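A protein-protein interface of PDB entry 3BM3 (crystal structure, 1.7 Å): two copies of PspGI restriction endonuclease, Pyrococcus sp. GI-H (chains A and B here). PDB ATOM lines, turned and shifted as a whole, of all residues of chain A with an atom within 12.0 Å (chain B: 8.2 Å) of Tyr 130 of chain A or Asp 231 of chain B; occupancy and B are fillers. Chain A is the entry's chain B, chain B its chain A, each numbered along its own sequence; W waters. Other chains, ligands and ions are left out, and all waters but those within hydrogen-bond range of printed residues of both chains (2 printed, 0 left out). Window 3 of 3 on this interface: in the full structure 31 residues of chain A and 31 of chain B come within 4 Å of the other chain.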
ATOM      1  N   VAL A 124      -4.112  -9.425 -11.718  1.00  0.00           N
ATOM      2  CA  VAL A 124      -4.926  -8.216 -11.821  1.00  0.00           C
ATOM      3  C   VAL A 124      -6.163  -8.481 -12.676  1.00  0.00           C
ATOM      4  O   VAL A 124      -6.074  -9.019 -13.788  1.00  0.00           O
ATOM      5  CB  VAL A 124      -4.115  -7.060 -12.415  1.00  0.00           C
ATOM      6  CG1 VAL A 124      -5.009  -5.864 -12.737  1.00  0.00           C
ATOM      7  CG2 VAL A 124      -2.984  -6.656 -11.463  1.00  0.00           C
ATOM      8  N   ILE A 125      -7.317  -8.121 -12.128  1.00  0.00           N
ATOM      9  CA  ILE A 125      -8.574  -8.151 -12.848  1.00  0.00           C
ATOM     10  C   ILE A 125      -8.766  -6.743 -13.384  1.00  0.00           C
ATOM     11  O   ILE A 125      -8.902  -5.800 -12.606  1.00  0.00           O
ATOM     12  CB  ILE A 125      -9.743  -8.549 -11.928  1.00  0.00           C
ATOM     13  CG1 ILE A 125      -9.521  -9.961 -11.364  1.00  0.00           C
ATOM     14  CG2 ILE A 125     -11.093  -8.443 -12.678  1.00  0.00           C
ATOM     15  CD1 ILE A 125     -10.552 -10.376 -10.306  1.00  0.00           C
ATOM     16  N   LYS A 126      -8.738  -6.601 -14.698  1.00  0.00           N
ATOM     17  CA  LYS A 126      -8.849  -5.265 -15.314  1.00  0.00           C
ATOM     18  C   LYS A 126     -10.263  -4.778 -15.154  1.00  0.00           C
ATOM     19  O   LYS A 126     -11.219  -5.523 -15.338  1.00  0.00           O
ATOM     20  CB  LYS A 126      -8.461  -5.259 -16.795  1.00  0.00           C
ATOM     21  CG  LYS A 126      -6.986  -5.544 -17.021  1.00  0.00           C
ATOM     22  CD  LYS A 126      -6.177  -4.286 -17.306  1.00  0.00           C
ATOM     23  CE  LYS A 126      -4.670  -4.602 -17.410  1.00  0.00           C
ATOM     24  NZ  LYS A 126      -4.350  -5.706 -18.357  1.00  0.00           N
ATOM     25  N   ILE A 127     -10.385  -3.517 -14.786  1.00  0.00           N
ATOM     26  CA  ILE A 127     -11.683  -2.870 -14.639  1.00  0.00           C
ATOM     27  C   ILE A 127     -11.950  -2.011 -15.878  1.00  0.00           C
ATOM     28  O   ILE A 127     -13.071  -1.939 -16.339  1.00  0.00           O
ATOM     29  CB  ILE A 127     -11.713  -2.023 -13.341  1.00  0.00           C
ATOM     30  CG1 ILE A 127     -11.404  -2.868 -12.088  1.00  0.00           C
ATOM     31  CG2 ILE A 127     -13.039  -1.297 -13.196  1.00  0.00           C
ATOM     32  CD1 ILE A 127     -12.328  -4.095 -11.879  1.00  0.00           C
ATOM     33  N   TYR A 128     -10.899  -1.356 -16.376  1.00  0.00           N
ATOM     34  CA  TYR A 128     -10.941  -0.563 -17.583  1.00  0.00           C
ATOM     35  C   TYR A 128      -9.884  -1.151 -18.494  1.00  0.00           C
ATOM     36  O   TYR A 128      -8.733  -1.286 -18.113  1.00  0.00           O
ATOM     37  CB  TYR A 128     -10.576   0.880 -17.280  1.00  0.00           C
ATOM     38  CG  TYR A 128     -11.352   1.439 -16.117  1.00  0.00           C
ATOM     39  CD1 TYR A 128     -12.604   2.014 -16.311  1.00  0.00           C
ATOM     40  CD2 TYR A 128     -10.830   1.417 -14.833  1.00  0.00           C
ATOM     41  CE1 TYR A 128     -13.328   2.540 -15.231  1.00  0.00           C
ATOM     42  CE2 TYR A 128     -11.537   1.919 -13.775  1.00  0.00           C
ATOM     43  CZ  TYR A 128     -12.782   2.470 -13.966  1.00  0.00           C
ATOM     44  OH  TYR A 128     -13.485   2.975 -12.903  1.00  0.00           O
ATOM     45  N   ASP A 129     -10.269  -1.497 -19.707  1.00  0.00           N
ATOM     46  CA  ASP A 129      -9.305  -2.159 -20.581  1.00  0.00           C
ATOM     47  C   ASP A 129      -8.140  -1.227 -20.945  1.00  0.00           C
ATOM     48  O   ASP A 129      -7.041  -1.696 -21.226  1.00  0.00           O
ATOM     49  CB  ASP A 129      -9.999  -2.743 -21.812  1.00  0.00           C
ATOM     50  CG  ASP A 129     -10.708  -4.046 -21.502  1.00  0.00           C
ATOM     51  OD1 ASP A 129     -10.356  -4.709 -20.489  1.00  0.00           O
ATOM     52  OD2 ASP A 129     -11.607  -4.423 -22.263  1.00  0.00           O
ATOM     53  N   TYR A 130      -8.371   0.077 -20.870  1.00  0.00           N
ATOM     54  CA  TYR A 130      -7.344   1.081 -21.191  1.00  0.00           C
ATOM     55  C   TYR A 130      -6.538   1.566 -19.990  1.00  0.00           C
ATOM     56  O   TYR A 130      -5.754   2.484 -20.123  1.00  0.00           O
ATOM     57  CB  TYR A 130      -7.986   2.289 -21.874  1.00  0.00           C
ATOM     58  CG  TYR A 130      -9.270   2.684 -21.223  1.00  0.00           C
ATOM     59  CD1 TYR A 130     -10.486   2.192 -21.690  1.00  0.00           C
ATOM     60  CD2 TYR A 130      -9.277   3.510 -20.121  1.00  0.00           C
ATOM     61  CE1 TYR A 130     -11.680   2.542 -21.070  1.00  0.00           C
ATOM     62  CE2 TYR A 130     -10.456   3.862 -19.501  1.00  0.00           C
ATOM     63  CZ  TYR A 130     -11.656   3.384 -19.991  1.00  0.00           C
ATOM     64  OH  TYR A 130     -12.823   3.733 -19.368  1.00  0.00           O
ATOM     65  N   ILE A 131      -6.735   0.964 -18.815  1.00  0.00           N
ATOM     66  CA  ILE A 131      -5.925   1.281 -17.638  1.00  0.00           C
ATOM     67  C   ILE A 131      -5.263  -0.006 -17.171  1.00  0.00           C
ATOM     68  O   ILE A 131      -5.925  -1.020 -16.978  1.00  0.00           O
ATOM     69  CB  ILE A 131      -6.771   1.954 -16.510  1.00  0.00           C
ATOM     70  CG1 ILE A 131      -7.347   3.277 -17.006  1.00  0.00           C
ATOM     71  CG2 ILE A 131      -5.928   2.189 -15.254  1.00  0.00           C
ATOM     72  CD1 ILE A 131      -7.931   4.130 -15.921  1.00  0.00           C
ATOM     73  N   THR A 132      -3.944   0.023 -17.025  1.00  0.00           N
ATOM     74  CA  THR A 132      -3.203  -1.201 -16.751  1.00  0.00           C
ATOM     75  C   THR A 132      -3.541  -1.675 -15.341  1.00  0.00           C
ATOM     76  O   THR A 132      -3.635  -2.868 -15.065  1.00  0.00           O
ATOM     77  CB  THR A 132      -1.684  -1.014 -17.009  1.00  0.00           C
ATOM     78  OG1 THR A 132      -1.164   0.016 -16.170  1.00  0.00           O
ATOM     79  CG2 THR A 132      -1.465  -0.578 -18.432  1.00  0.00           C
ATOM     80  N   GLU A 133      -3.777  -0.717 -14.457  1.00  0.00           N
ATOM     81  CA  GLU A 133      -4.066  -1.001 -13.069  1.00  0.00           C
ATOM     82  C   GLU A 133      -5.518  -1.466 -12.891  1.00  0.00           C
ATOM     83  O   GLU A 133      -6.432  -0.891 -13.474  1.00  0.00           O
ATOM     84  CB  GLU A 133      -3.778   0.241 -12.229  1.00  0.00           C
ATOM     85  CG  GLU A 133      -2.294   0.664 -12.228  1.00  0.00           C
ATOM     86  CD  GLU A 133      -1.841   1.517 -13.430  1.00  0.00           C
ATOM     87  OE1 GLU A 133      -2.680   2.159 -14.116  1.00  0.00           O
ATOM     88  OE2 GLU A 133      -0.606   1.556 -13.675  1.00  0.00           O
ATOM     89  N   GLY A 134      -5.715  -2.500 -12.077  1.00  0.00           N
ATOM     90  CA  GLY A 134      -7.044  -2.997 -11.762  1.00  0.00           C
ATOM     91  C   GLY A 134      -7.156  -3.449 -10.318  1.00  0.00           C
ATOM     92  O   GLY A 134      -6.507  -2.923  -9.405  1.00  0.00           O
ATOM     93  N   GLU A 135      -7.997  -4.439 -10.111  1.00  0.00           N
ATOM     94  CA  GLU A 135      -8.220  -5.004  -8.796  1.00  0.00           C
ATOM     95  C   GLU A 135      -7.427  -6.300  -8.702  1.00  0.00           C
ATOM     96  O   GLU A 135      -7.342  -7.038  -9.668  1.00  0.00           O
ATOM     97  CB  GLU A 135      -9.705  -5.239  -8.535  1.00  0.00           C
ATOM     98  CG  GLU A 135     -10.475  -3.920  -8.453  1.00  0.00           C
ATOM     99  CD  GLU A 135      -9.902  -3.007  -7.368  1.00  0.00           C
ATOM    100  OE1 GLU A 135      -9.890  -3.439  -6.193  1.00  0.00           O
ATOM    101  OE2 GLU A 135      -9.414  -1.901  -7.690  1.00  0.00           O
ATOM    102  N   ILE A 176     -15.921  -2.210  -6.339  1.00  0.00           N
ATOM    103  CA  ILE A 176     -15.402  -1.994  -7.683  1.00  0.00           C
ATOM    104  C   ILE A 176     -15.675  -3.202  -8.598  1.00  0.00           C
ATOM    105  O   ILE A 176     -16.134  -3.071  -9.759  1.00  0.00           O
ATOM    106  CB  ILE A 176     -13.915  -1.694  -7.657  1.00  0.00           C
ATOM    107  CG1 ILE A 176     -13.674  -0.374  -6.898  1.00  0.00           C
ATOM    108  CG2 ILE A 176     -13.357  -1.698  -9.085  1.00  0.00           C
ATOM    109  CD1 ILE A 176     -12.242  -0.129  -6.465  1.00  0.00           C
ATOM    110  N   ASN A 179     -19.422  -3.668  -9.207  1.00  0.00           N
ATOM    111  CA  ASN A 179     -19.886  -2.649 -10.115  1.00  0.00           C
ATOM    112  C   ASN A 179     -19.641  -3.099 -11.540  1.00  0.00           C
ATOM    113  O   ASN A 179     -20.469  -2.859 -12.436  1.00  0.00           O
ATOM    114  CB  ASN A 179     -19.165  -1.340  -9.835  1.00  0.00           C
ATOM    115  CG  ASN A 179     -19.710  -0.208 -10.610  1.00  0.00           C
ATOM    116  OD1 ASN A 179     -20.935  -0.093 -10.768  1.00  0.00           O
ATOM    117  ND2 ASN A 179     -18.834   0.665 -11.087  1.00  0.00           N
ATOM    118  N   LYS A 180     -18.496  -3.726 -11.757  1.00  0.00           N
ATOM    119  CA  LYS A 180     -18.088  -4.170 -13.079  1.00  0.00           C
ATOM    120  C   LYS A 180     -18.718  -5.481 -13.483  1.00  0.00           C
ATOM    121  O   LYS A 180     -19.231  -5.616 -14.612  1.00  0.00           O
ATOM    122  CB  LYS A 180     -16.574  -4.307 -13.123  1.00  0.00           C
ATOM    123  CG  LYS A 180     -16.038  -4.950 -14.382  1.00  0.00           C
ATOM    124  CD  LYS A 180     -15.513  -3.967 -15.323  1.00  0.00           C
ATOM    125  CE  LYS A 180     -14.794  -4.673 -16.469  1.00  0.00           C
ATOM    126  NZ  LYS A 180     -14.830  -3.732 -17.592  1.00  0.00           N
ATOM    127  N   PHE A 181     -18.633  -6.456 -12.589  1.00  0.00           N
ATOM    128  CA  PHE A 181     -18.949  -7.831 -12.928  1.00  0.00           C
ATOM    129  C   PHE A 181     -20.295  -8.321 -12.435  1.00  0.00           C
ATOM    130  O   PHE A 181     -20.713  -9.436 -12.797  1.00  0.00           O
ATOM    131  CB  PHE A 181     -17.865  -8.743 -12.435  1.00  0.00           C
ATOM    132  CG  PHE A 181     -16.576  -8.529 -13.109  1.00  0.00           C
ATOM    133  CD1 PHE A 181     -16.366  -9.001 -14.393  1.00  0.00           C
ATOM    134  CD2 PHE A 181     -15.563  -7.816 -12.492  1.00  0.00           C
ATOM    135  CE1 PHE A 181     -15.185  -8.805 -15.042  1.00  0.00           C
ATOM    136  CE2 PHE A 181     -14.380  -7.642 -13.132  1.00  0.00           C
ATOM    137  CZ  PHE A 181     -14.202  -8.134 -14.437  1.00  0.00           C
ATOM    138  N   ILE B 198      -3.848   7.639 -11.020  1.00  0.00           N
ATOM    139  CA  ILE B 198      -4.994   7.799 -11.923  1.00  0.00           C
ATOM    140  C   ILE B 198      -6.036   6.738 -11.675  1.00  0.00           C
ATOM    141  O   ILE B 198      -7.216   7.047 -11.637  1.00  0.00           O
ATOM    142  CB  ILE B 198      -4.541   7.802 -13.386  1.00  0.00           C
ATOM    143  CG1 ILE B 198      -5.717   7.975 -14.332  1.00  0.00           C
ATOM    144  CG2 ILE B 198      -3.833   6.509 -13.730  1.00  0.00           C
ATOM    145  CD1 ILE B 198      -5.273   8.038 -15.834  1.00  0.00           C
ATOM    146  N   ILE B 202     -10.048   7.428 -10.878  1.00  0.00           N
ATOM    147  CA  ILE B 202     -11.096   6.933 -11.771  1.00  0.00           C
ATOM    148  C   ILE B 202     -11.997   5.916 -11.071  1.00  0.00           C
ATOM    149  O   ILE B 202     -13.210   6.027 -11.086  1.00  0.00           O
ATOM    150  CB  ILE B 202     -10.473   6.346 -13.043  1.00  0.00           C
ATOM    151  CG1 ILE B 202      -9.756   7.463 -13.813  1.00  0.00           C
ATOM    152  CG2 ILE B 202     -11.542   5.699 -13.892  1.00  0.00           C
ATOM    153  CD1 ILE B 202      -8.983   6.956 -15.007  1.00  0.00           C
ATOM    154  N   ASP B 206     -16.041   6.284 -10.101  1.00  0.00           N
ATOM    155  CA  ASP B 206     -16.980   5.340 -10.655  1.00  0.00           C
ATOM    156  C   ASP B 206     -17.657   4.513  -9.598  1.00  0.00           C
ATOM    157  O   ASP B 206     -18.578   3.743  -9.898  1.00  0.00           O
ATOM    158  CB  ASP B 206     -16.267   4.446 -11.661  1.00  0.00           C
ATOM    159  CG  ASP B 206     -16.097   5.112 -13.004  1.00  0.00           C
ATOM    160  OD1 ASP B 206     -16.870   6.054 -13.328  1.00  0.00           O
ATOM    161  OD2 ASP B 206     -15.206   4.670 -13.748  1.00  0.00           O
ATOM    162  N   GLU B 225      -1.914  12.583 -17.295  1.00  0.00           N
ATOM    163  CA  GLU B 225      -2.030  11.139 -17.439  1.00  0.00           C
ATOM    164  C   GLU B 225      -3.398  10.751 -17.969  1.00  0.00           C
ATOM    165  O   GLU B 225      -3.512   9.923 -18.871  1.00  0.00           O
ATOM    166  CB  GLU B 225      -1.792  10.425 -16.124  1.00  0.00           C
ATOM    167  CG  GLU B 225      -0.386  10.395 -15.678  1.00  0.00           C
ATOM    168  CD  GLU B 225      -0.227   9.568 -14.423  1.00  0.00           C
ATOM    169  OE1 GLU B 225      -0.892   8.515 -14.317  1.00  0.00           O
ATOM    170  OE2 GLU B 225       0.575   9.961 -13.559  1.00  0.00           O
ATOM    171  N   ILE B 226      -4.438  11.344 -17.400  1.00  0.00           N
ATOM    172  CA  ILE B 226      -5.789  11.095 -17.849  1.00  0.00           C
ATOM    173  C   ILE B 226      -5.931  11.446 -19.341  1.00  0.00           C
ATOM    174  O   ILE B 226      -6.457  10.663 -20.136  1.00  0.00           O
ATOM    175  CB  ILE B 226      -6.789  11.858 -16.952  1.00  0.00           C
ATOM    176  CG1 ILE B 226      -6.802  11.201 -15.564  1.00  0.00           C
ATOM    177  CG2 ILE B 226      -8.177  11.886 -17.574  1.00  0.00           C
ATOM    178  CD1 ILE B 226      -7.658  11.918 -14.491  1.00  0.00           C
ATOM    179  N   LYS B 227      -5.415  12.609 -19.709  1.00  0.00           N
ATOM    180  CA  LYS B 227      -5.514  13.096 -21.093  1.00  0.00           C
ATOM    181  C   LYS B 227      -4.756  12.212 -22.071  1.00  0.00           C
ATOM    182  O   LYS B 227      -5.078  12.188 -23.262  1.00  0.00           O
ATOM    183  CB  LYS B 227      -5.018  14.537 -21.177  1.00  0.00           C
ATOM    184  CG  LYS B 227      -5.997  15.542 -20.569  1.00  0.00           C
ATOM    185  CD  LYS B 227      -5.543  16.962 -20.843  1.00  0.00           C
ATOM    186  CE  LYS B 227      -6.440  18.032 -20.224  1.00  0.00           C
ATOM    187  NZ  LYS B 227      -5.792  19.417 -20.339  1.00  0.00           N
ATOM    188  N   ARG B 228      -3.751  11.495 -21.573  1.00  0.00           N
ATOM    189  CA  ARG B 228      -2.915  10.623 -22.393  1.00  0.00           C
ATOM    190  C   ARG B 228      -3.508   9.236 -22.576  1.00  0.00           C
ATOM    191  O   ARG B 228      -2.937   8.403 -23.289  1.00  0.00           O
ATOM    192  CB  ARG B 228      -1.501  10.523 -21.812  1.00  0.00           C
ATOM    193  CG  ARG B 228      -0.714  11.829 -21.940  1.00  0.00           C
ATOM    194  CD  ARG B 228       0.642  11.741 -21.267  1.00  0.00           C
ATOM    195  NE  ARG B 228       1.651  11.103 -22.120  1.00  0.00           N
ATOM    196  CZ  ARG B 228       2.520  11.738 -22.916  1.00  0.00           C
ATOM    197  NH1 ARG B 228       2.534  13.074 -23.023  1.00  0.00           N
ATOM    198  NH2 ARG B 228       3.395  11.020 -23.626  1.00  0.00           N
ATOM    199  N   ILE B 229      -4.640   8.961 -21.929  1.00  0.00           N
ATOM    200  CA  ILE B 229      -5.376   7.750 -22.251  1.00  0.00           C
ATOM    201  C   ILE B 229      -5.993   8.022 -23.633  1.00  0.00           C
ATOM    202  O   ILE B 229      -6.745   8.983 -23.810  1.00  0.00           O
ATOM    203  CB  ILE B 229      -6.438   7.404 -21.199  1.00  0.00           C
ATOM    204  CG1 ILE B 229      -5.764   7.101 -19.859  1.00  0.00           C
ATOM    205  CG2 ILE B 229      -7.258   6.213 -21.683  1.00  0.00           C
ATOM    206  CD1 ILE B 229      -6.727   7.017 -18.656  1.00  0.00           C
ATOM    207  N   SER B 230      -5.605   7.247 -24.631  1.00  0.00           N
ATOM    208  CA  SER B 230      -5.995   7.576 -26.017  1.00  0.00           C
ATOM    209  C   SER B 230      -7.149   6.741 -26.516  1.00  0.00           C
ATOM    210  O   SER B 230      -7.664   6.980 -27.601  1.00  0.00           O
ATOM    211  CB  SER B 230      -4.802   7.433 -26.964  1.00  0.00           C
ATOM    212  OG  SER B 230      -3.741   8.254 -26.509  1.00  0.00           O
ATOM    213  N   ASP B 231      -7.549   5.754 -25.737  1.00  0.00           N
ATOM    214  CA  ASP B 231      -8.686   4.929 -26.102  1.00  0.00           C
ATOM    215  C   ASP B 231      -9.907   5.845 -26.139  1.00  0.00           C
ATOM    216  O   ASP B 231     -10.263   6.436 -25.122  1.00  0.00           O
ATOM    217  CB  ASP B 231      -8.842   3.797 -25.084  1.00  0.00           C
ATOM    218  CG  ASP B 231      -9.995   2.887 -25.386  1.00  0.00           C
ATOM    219  OD1 ASP B 231     -10.951   3.314 -26.068  1.00  0.00           O
ATOM    220  OD2 ASP B 231      -9.942   1.713 -24.939  1.00  0.00           O
ATOM    221  N   PRO B 232     -10.519   6.022 -27.316  1.00  0.00           N
ATOM    222  CA  PRO B 232     -11.649   6.966 -27.397  1.00  0.00           C
ATOM    223  C   PRO B 232     -12.887   6.584 -26.583  1.00  0.00           C
ATOM    224  O   PRO B 232     -13.778   7.403 -26.413  1.00  0.00           O
ATOM    225  CB  PRO B 232     -11.987   6.986 -28.891  1.00  0.00           C
ATOM    226  CG  PRO B 232     -11.385   5.743 -29.459  1.00  0.00           C
ATOM    227  CD  PRO B 232     -10.203   5.410 -28.620  1.00  0.00           C
ATOM    228  N   ASN B 233     -12.950   5.355 -26.084  1.00  0.00           N
ATOM    229  CA  ASN B 233     -14.053   4.932 -25.265  1.00  0.00           C
ATOM    230  C   ASN B 233     -13.930   5.480 -23.843  1.00  0.00           C
ATOM    231  O   ASN B 233     -14.843   5.299 -23.024  1.00  0.00           O
ATOM    232  CB  ASN B 233     -14.109   3.412 -25.194  1.00  0.00           C
ATOM    233  CG  ASN B 233     -14.438   2.770 -26.539  1.00  0.00           C
ATOM    234  OD1 ASN B 233     -15.098   3.373 -27.386  1.00  0.00           O
ATOM    235  ND2 ASN B 233     -13.962   1.555 -26.740  1.00  0.00           N
ATOM    236  N   PHE B 234     -12.781   6.078 -23.538  1.00  0.00           N
ATOM    237  CA  PHE B 234     -12.568   6.700 -22.243  1.00  0.00           C
ATOM    238  C   PHE B 234     -13.012   8.143 -22.327  1.00  0.00           C
ATOM    239  O   PHE B 234     -12.467   8.920 -23.122  1.00  0.00           O
ATOM    240  CB  PHE B 234     -11.108   6.636 -21.871  1.00  0.00           C
ATOM    241  CG  PHE B 234     -10.789   7.333 -20.597  1.00  0.00           C
ATOM    242  CD1 PHE B 234     -11.445   6.996 -19.432  1.00  0.00           C
ATOM    243  CD2 PHE B 234      -9.829   8.334 -20.555  1.00  0.00           C
ATOM    244  CE1 PHE B 234     -11.152   7.625 -18.260  1.00  0.00           C
ATOM    245  CE2 PHE B 234      -9.540   8.978 -19.351  1.00  0.00           C
ATOM    246  CZ  PHE B 234     -10.200   8.599 -18.208  1.00  0.00           C
ATOM    247  N   ASN B 235     -14.019   8.477 -21.520  1.00  0.00           N
ATOM    248  CA  ASN B 235     -14.587   9.816 -21.472  1.00  0.00           C
ATOM    249  C   ASN B 235     -13.857  10.605 -20.380  1.00  0.00           C
ATOM    250  O   ASN B 235     -14.267  10.620 -19.236  1.00  0.00           O
ATOM    251  CB  ASN B 235     -16.082   9.735 -21.151  1.00  0.00           C
ATOM    252  CG  ASN B 235     -16.753  11.114 -21.095  1.00  0.00           C
ATOM    253  OD1 ASN B 235     -16.120  12.138 -21.345  1.00  0.00           O
ATOM    254  ND2 ASN B 235     -18.046  11.133 -20.771  1.00  0.00           N
ATOM    255  N   GLU B 236     -12.744  11.227 -20.745  1.00  0.00           N
ATOM    256  CA  GLU B 236     -11.909  11.944 -19.771  1.00  0.00           C
ATOM    257  C   GLU B 236     -12.669  13.070 -19.070  1.00  0.00           C
ATOM    258  O   GLU B 236     -12.476  13.299 -17.869  1.00  0.00           O
ATOM    259  CB  GLU B 236     -10.641  12.506 -20.442  1.00  0.00           C
ATOM    260  CG  GLU B 236     -10.908  13.544 -21.532  1.00  0.00           C
ATOM    261  CD  GLU B 236      -9.699  13.833 -22.423  1.00  0.00           C
ATOM    262  OE1 GLU B 236      -9.216  12.903 -23.113  1.00  0.00           O
ATOM    263  OE2 GLU B 236      -9.257  14.999 -22.460  1.00  0.00           O
ATOM    264  N   LYS B 238     -15.711  13.452 -18.080  1.00  0.00           N
ATOM    265  CA  LYS B 238     -16.520  12.957 -16.982  1.00  0.00           C
ATOM    266  C   LYS B 238     -15.716  12.919 -15.678  1.00  0.00           C
ATOM    267  O   LYS B 238     -16.225  13.248 -14.602  1.00  0.00           O
ATOM    268  CB  LYS B 238     -17.081  11.573 -17.371  1.00  0.00           C
ATOM    269  CG  LYS B 238     -17.392  10.608 -16.226  1.00  0.00           C
ATOM    270  CD  LYS B 238     -18.172   9.390 -16.733  1.00  0.00           C
ATOM    271  CE  LYS B 238     -17.405   8.603 -17.791  1.00  0.00           C
ATOM    272  NZ  LYS B 238     -17.943   7.230 -18.091  1.00  0.00           N
ATOM    273  N   TYR B 239     -14.451  12.542 -15.781  1.00  0.00           N
ATOM    274  CA  TYR B 239     -13.606  12.390 -14.625  1.00  0.00           C
ATOM    275  C   TYR B 239     -12.893  13.665 -14.241  1.00  0.00           C
ATOM    276  O   TYR B 239     -12.813  14.015 -13.058  1.00  0.00           O
ATOM    277  CB  TYR B 239     -12.577  11.313 -14.907  1.00  0.00           C
ATOM    278  CG  TYR B 239     -13.235   9.996 -15.113  1.00  0.00           C
ATOM    279  CD1 TYR B 239     -13.714   9.256 -14.026  1.00  0.00           C
ATOM    280  CD2 TYR B 239     -13.413   9.479 -16.387  1.00  0.00           C
ATOM    281  CE1 TYR B 239     -14.342   8.083 -14.203  1.00  0.00           C
ATOM    282  CE2 TYR B 239     -14.021   8.260 -16.572  1.00  0.00           C
ATOM    283  CZ  TYR B 239     -14.490   7.569 -15.470  1.00  0.00           C
ATOM    284  OH  TYR B 239     -15.083   6.347 -15.668  1.00  0.00           O
HETATM  285  O   HOH W   1     -14.391   4.981 -17.888  1.00  0.00           O
HETATM  286  O   HOH W   2     -19.848   3.119 -12.283  1.00  0.00           O
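The side-chain carboxylate (OD2) of Asp 206 of chain B lies within hydrogen-bond range of the side-chain hydroxyl (OH) of Tyr 239 of chain B, 2.6 Å away. The backbone NH (N) of Asn 233 of chain B is in hydrogen-bond range of the side-chain carboxylate (OD1) of Asp 231 of chain B (2.9 Å).
Printed residues of chain B that touch a printed residue of chain A: Ile 202, Asp 206, Ile 229, Asp 231 and Phe 234. Hydrophobic or aromatic side chains of chain B within 4 Å of the printed part of chain A: Ile 202, Ile 229 and Phe 234. Of the 16 printed residues of chain A, 4 touch a printed residue of chain B. Along chain A the printed residues that touch a printed residue of chain B span positions 128 to 179. Among the printed residues, 7 pairs touch across the chains.
Ile 127 of chain A touches none of the printed residues of chain B. Printed residues of chain B within 4 Å of Tyr 128 of chain A: Ile 202 (3.5 Å) and Asp 206 (2.6 Å). Of chain B, only Ile 229, Asp 231 and Phe 234 come within 4 Å of Tyr 130 of chain A. Of the printed residues of chain B, Ile 131 of chain A touches Ile 202. Printed residues of chain B within 4 Å of Asn 179 of chain A: Asp 206 (3.3 Å). Lys 180 of chain A touches none of the printed residues of chain B. Of the printed residues of chain A, Ile 202 of chain B touches Tyr 128 (3.5 Å) and Ile 131 (3.2 Å). Printed residues of chain A within 4 Å of Asp 206 of chain B: Tyr 128 (2.6 Å) and Asn 179 (3.3 Å). Of chain A, only Tyr 130 (3.3 Å) comes within 4 Å of Asp 231 of chain B. Pro 232 of chain B touches none of the printed residues of chain A. No residue of chain A comes within 4 Å of Asn 233 of chain B. Phe 234 of chain B touches just one residue of chain A: Tyr 130 (3.3 Å). The nearest residue of chain A that does not touch Asp 231 of chain B is Asp 129 of chain A (5.3 Å). The nearest printed residue of chain B that does not touch Asn 179 of chain A is Ile 202 of chain B (7.8 Å).
Among the printed residues, merely in contact across the chains: Ile 131 of chain A with Ile 202 of chain B (3.2 Å), Tyr 130 of chain A with Phe 234 of chain B (3.3 Å), Tyr 130 of chain A with Asp 231 of chain B (3.3 Å), Tyr 128 of chain A with Ile 202 of chain B (3.5 Å) and Tyr 130 of chain A with Ile 229 of chain B (3.7 Å).
No position is printed for both chains. Of the 7 pairs that touch across the chains among the printed residues, none has its exchanged pair printed and touching as well.
OD2 of Asp 206 of chain B lies within hydrogen-bond range of OH of Tyr 128 of chain A. The backbone carbonyl oxygen of Asp 206 of chain B lies within hydrogen-bond range of the side-chain amide nitrogen of Asn 179 of chain A (3.3 Å).
Water W1 lies within hydrogen-bond range of OH of Tyr 130 of chain A (2.5 Å) and OH of Tyr 239 of chain B (2.7 Å). Water W2 bridges O of Asp 206 of chain B and ND2 of Asn 179 of chain A.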
